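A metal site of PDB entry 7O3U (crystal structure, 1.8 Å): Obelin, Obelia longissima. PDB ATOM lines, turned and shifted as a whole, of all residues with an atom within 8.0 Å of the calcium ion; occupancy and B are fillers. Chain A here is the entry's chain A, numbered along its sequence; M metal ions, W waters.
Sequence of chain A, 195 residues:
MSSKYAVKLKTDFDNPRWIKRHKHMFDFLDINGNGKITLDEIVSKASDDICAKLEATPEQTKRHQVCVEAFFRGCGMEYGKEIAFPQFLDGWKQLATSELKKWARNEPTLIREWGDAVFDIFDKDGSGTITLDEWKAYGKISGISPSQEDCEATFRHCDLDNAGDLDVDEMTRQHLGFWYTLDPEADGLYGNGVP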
ATOM      1  N   PHE A  26       4.948  15.070  10.438  1.00  0.00           N
ATOM      2  CA  PHE A  26       5.149  14.150   9.301  1.00  0.00           C
ATOM      3  C   PHE A  26       6.628  13.845   9.107  1.00  0.00           C
ATOM      4  O   PHE A  26       7.002  12.679   8.884  1.00  0.00           O
ATOM      5  CB  PHE A  26       4.556  14.758   8.025  1.00  0.00           C
ATOM      6  CG  PHE A  26       4.701  13.881   6.768  1.00  0.00           C
ATOM      7  CD1 PHE A  26       3.725  12.917   6.447  1.00  0.00           C
ATOM      8  CD2 PHE A  26       5.789  14.021   5.938  1.00  0.00           C
ATOM      9  CE1 PHE A  26       3.845  12.122   5.286  1.00  0.00           C
ATOM     10  CE2 PHE A  26       5.936  13.214   4.766  1.00  0.00           C
ATOM     11  CZ  PHE A  26       4.954  12.282   4.451  1.00  0.00           C
ATOM     12  N   ASP A  27       7.474  14.874   9.063  1.00  0.00           N
ATOM     13  CA  ASP A  27       8.902  14.619   8.917  1.00  0.00           C
ATOM     14  C   ASP A  27       9.437  13.744  10.023  1.00  0.00           C
ATOM     15  O   ASP A  27      10.292  12.880   9.780  1.00  0.00           O
ATOM     16  CB  ASP A  27       9.684  15.945   8.878  1.00  0.00           C
ATOM     17  CG  ASP A  27       9.320  16.784   7.671  1.00  0.00           C
ATOM     18  OD1 ASP A  27       8.670  16.248   6.745  1.00  0.00           O
ATOM     19  OD2 ASP A  27       9.695  17.963   7.646  1.00  0.00           O
ATOM     20  N   LEU A  29       7.693  11.522  11.556  1.00  0.00           N
ATOM     21  CA  LEU A  29       7.310  10.144  11.209  1.00  0.00           C
ATOM     22  C   LEU A  29       8.100   9.622  10.006  1.00  0.00           C
ATOM     23  O   LEU A  29       8.373   8.423   9.924  1.00  0.00           O
ATOM     24  CB  LEU A  29       5.809  10.064  10.936  1.00  0.00           C
ATOM     25  CG  LEU A  29       4.926  10.337  12.145  1.00  0.00           C
ATOM     26  CD1 LEU A  29       3.447  10.336  11.680  1.00  0.00           C
ATOM     27  CD2 LEU A  29       5.101   9.273  13.252  1.00  0.00           C
ATOM     28  N   ASP A  30       8.415  10.507   9.062  1.00  0.00           N
ATOM     29  CA  ASP A  30       9.223  10.093   7.880  1.00  0.00           C
ATOM     30  C   ASP A  30      10.674  10.005   8.371  1.00  0.00           C
ATOM     31  O   ASP A  30      11.452  10.941   8.110  1.00  0.00           O
ATOM     32  CB  ASP A  30       9.073  11.084   6.722  1.00  0.00           C
ATOM     33  CG  ASP A  30       9.958  10.753   5.526  1.00  0.00           C
ATOM     34  OD1 ASP A  30      10.217   9.561   5.300  1.00  0.00           O
ATOM     35  OD2 ASP A  30      10.384  11.701   4.843  1.00  0.00           O
ATOM     36  N   ILE A  31      11.019   8.903   9.056  1.00  0.00           N
ATOM     37  CA  ILE A  31      12.350   8.783   9.649  1.00  0.00           C
ATOM     38  C   ILE A  31      13.417   8.638   8.568  1.00  0.00           C
ATOM     39  O   ILE A  31      14.535   9.134   8.702  1.00  0.00           O
ATOM     40  CB  ILE A  31      12.395   7.606  10.643  1.00  0.00           C
ATOM     41  CG1 ILE A  31      13.700   7.628  11.457  1.00  0.00           C
ATOM     42  CG2 ILE A  31      12.206   6.276   9.933  1.00  0.00           C
ATOM     43  CD1 ILE A  31      13.575   8.470  12.782  1.00  0.00           C
ATOM     44  N   ASN A  32      13.094   7.948   7.490  1.00  0.00           N
ATOM     45  CA  ASN A  32      14.073   7.732   6.424  1.00  0.00           C
ATOM     46  C   ASN A  32      14.128   8.882   5.432  1.00  0.00           C
ATOM     47  O   ASN A  32      14.945   8.842   4.486  1.00  0.00           O
ATOM     48  CB  ASN A  32      13.795   6.384   5.741  1.00  0.00           C
ATOM     49  CG  ASN A  32      12.692   6.444   4.713  1.00  0.00           C
ATOM     50  OD1 ASN A  32      11.900   7.373   4.689  1.00  0.00           O
ATOM     51  ND2 ASN A  32      12.673   5.439   3.823  1.00  0.00           N
ATOM     52  N   GLY A  33      13.337   9.922   5.622  1.00  0.00           N
ATOM     53  CA  GLY A  33      13.499  11.124   4.838  1.00  0.00           C
ATOM     54  C   GLY A  33      13.071  11.022   3.391  1.00  0.00           C
ATOM     55  O   GLY A  33      13.479  11.857   2.574  1.00  0.00           O
ATOM     56  N   ASN A  34      12.271  10.034   3.022  1.00  0.00           N
ATOM     57  CA  ASN A  34      11.866   9.933   1.621  1.00  0.00           C
ATOM     58  C   ASN A  34      10.519  10.593   1.326  1.00  0.00           C
ATOM     59  O   ASN A  34      10.064  10.548   0.178  1.00  0.00           O
ATOM     60  CB  ASN A  34      11.866   8.472   1.157  1.00  0.00           C
ATOM     61  CG  ASN A  34      10.790   7.666   1.768  1.00  0.00           C
ATOM     62  OD1 ASN A  34       9.946   8.160   2.546  1.00  0.00           O
ATOM     63  ND2 ASN A  34      10.788   6.383   1.410  1.00  0.00           N
ATOM     64  N   GLY A  35       9.848  11.166   2.330  1.00  0.00           N
ATOM     65  CA  GLY A  35       8.629  11.883   2.036  1.00  0.00           C
ATOM     66  C   GLY A  35       7.395  11.024   1.993  1.00  0.00           C
ATOM     67  O   GLY A  35       6.327  11.520   1.563  1.00  0.00           O
ATOM     68  N   LYS A  36       7.495   9.757   2.453  1.00  0.00           N
ATOM     69  CA  LYS A  36       6.348   8.842   2.460  1.00  0.00           C
ATOM     70  C   LYS A  36       6.310   8.098   3.791  1.00  0.00           C
ATOM     71  O   LYS A  36       7.346   7.646   4.285  1.00  0.00           O
ATOM     72  CB  LYS A  36       6.420   7.790   1.352  1.00  0.00           C
ATOM     73  CG  LYS A  36       6.536   8.343  -0.063  1.00  0.00           C
ATOM     74  CD  LYS A  36       6.617   7.157  -1.039  1.00  0.00           C
ATOM     75  CE  LYS A  36       7.971   6.401  -0.942  1.00  0.00           C
ATOM     76  NZ  LYS A  36       8.037   5.386  -2.068  1.00  0.00           N
ATOM     77  N   ILE A  37       5.129   7.917   4.323  1.00  0.00           N
ATOM     78  CA  ILE A  37       4.990   7.118   5.523  1.00  0.00           C
ATOM     79  C   ILE A  37       3.878   6.099   5.297  1.00  0.00           C
ATOM     80  O   ILE A  37       3.058   6.261   4.398  1.00  0.00           O
ATOM     81  CB  ILE A  37       4.675   8.013   6.748  1.00  0.00           C
ATOM     82  CG1 ILE A  37       3.399   8.792   6.468  1.00  0.00           C
ATOM     83  CG2 ILE A  37       5.843   8.980   7.005  1.00  0.00           C
ATOM     84  CD1 ILE A  37       2.938   9.641   7.698  1.00  0.00           C
ATOM     85  N   THR A  38       3.873   5.027   6.084  1.00  0.00           N
ATOM     86  CA  THR A  38       2.833   3.998   5.984  1.00  0.00           C
ATOM     87  C   THR A  38       2.255   3.694   7.354  1.00  0.00           C
ATOM     88  O   THR A  38       2.965   3.737   8.361  1.00  0.00           O
ATOM     89  CB  THR A  38       3.351   2.682   5.393  1.00  0.00           C
ATOM     90  OG1 THR A  38       4.282   2.076   6.311  1.00  0.00           O
ATOM     91  CG2 THR A  38       4.069   2.964   4.084  1.00  0.00           C
ATOM     92  N   GLU A  41       4.495   1.280   9.206  1.00  0.00           N
ATOM     93  CA  GLU A  41       5.569   1.835  10.015  1.00  0.00           C
ATOM     94  C   GLU A  41       5.051   2.409  11.308  1.00  0.00           C
ATOM     95  O   GLU A  41       5.649   2.224  12.372  1.00  0.00           O
ATOM     96  CB  GLU A  41       6.307   2.929   9.241  1.00  0.00           C
ATOM     97  CG  GLU A  41       7.041   2.426   7.992  1.00  0.00           C
ATOM     98  CD  GLU A  41       7.406   3.567   7.040  1.00  0.00           C
ATOM     99  OE1 GLU A  41       6.756   4.639   7.080  1.00  0.00           O
ATOM    100  OE2 GLU A  41       8.393   3.415   6.299  1.00  0.00           O
ATOM    101  N   GLU A  82       1.352   4.021   0.825  1.00  0.00           N
ATOM    102  CA  GLU A  82       2.356   5.053   1.079  1.00  0.00           C
ATOM    103  C   GLU A  82       1.681   6.430   1.023  1.00  0.00           C
ATOM    104  O   GLU A  82       0.941   6.720   0.086  1.00  0.00           O
ATOM    105  CB  GLU A  82       3.515   4.958   0.065  1.00  0.00           C
ATOM    106  CG  GLU A  82       4.413   3.734   0.349  1.00  0.00           C
ATOM    107  CD  GLU A  82       5.495   3.528  -0.736  1.00  0.00           C
ATOM    108  OE1 GLU A  82       5.156   3.484  -1.944  1.00  0.00           O
ATOM    109  OE2 GLU A  82       6.685   3.473  -0.374  1.00  0.00           O
ATOM    110  N   ILE A  83       1.873   7.261   2.063  1.00  0.00           N
ATOM    111  CA  ILE A  83       1.229   8.554   2.172  1.00  0.00           C
ATOM    112  C   ILE A  83       2.288   9.651   2.119  1.00  0.00           C
ATOM    113  O   ILE A  83       3.241   9.618   2.929  1.00  0.00           O
ATOM    114  CB  ILE A  83       0.403   8.656   3.475  1.00  0.00           C
ATOM    115  CG1 ILE A  83      -0.760   7.673   3.369  1.00  0.00           C
ATOM    116  CG2 ILE A  83      -0.071  10.053   3.690  1.00  0.00           C
ATOM    117  CD1 ILE A  83      -1.790   8.046   2.261  1.00  0.00           C
HETATM  118 CA    CA M   1       9.602   7.560   4.778  1.00  0.00          CA
HETATM  119  O   HOH W   1       9.171   6.887   6.935  1.00  0.00           O
HETATM  120  O   HOH W   2       8.791   5.413   4.105  1.00  0.00           O
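The calcium ion is bound by OD1 of Asp 30. The calcium ion is bound by water W1, 2.3 Å away. The side-chain amide oxygen (OD1) of Asn 32 binds the calcium ion, at 2.3 Å. O of Lys 36 is bound to the calcium ion (2.3 Å). The calcium ion is bound by OD1 of Asn 34, 2.3 Å away. Water W2 binds the calcium ion. The calcium ion has six donor atoms within binding distance.
NZ of Lys 36 lies within salt-bridge range of OE2 of Glu 82 (2.9 Å). N of Gly 33 lies close to OD1 of Asp 30, 3.2 Å away. OD2 of Asp 30 is in hydrogen-bond range of N of Gly 35 (2.6 Å).
Water W1 lies within hydrogen-bond range of the side-chain carboxylate of Glu 41 (3.3 Å), the backbone carbonyl oxygen of Leu 29 (3.5 Å) and the backbone NH of Ile 31 (3.5 Å). Water W2 lies within hydrogen-bond range of the side-chain carboxylate of Glu 41 (3.0 Å) and the side-chain amide nitrogen of Asn 34 (3.5 Å).
Within 4 Å of the calcium ion: Asp 30, Asn 32, Asn 34 and Lys 36.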
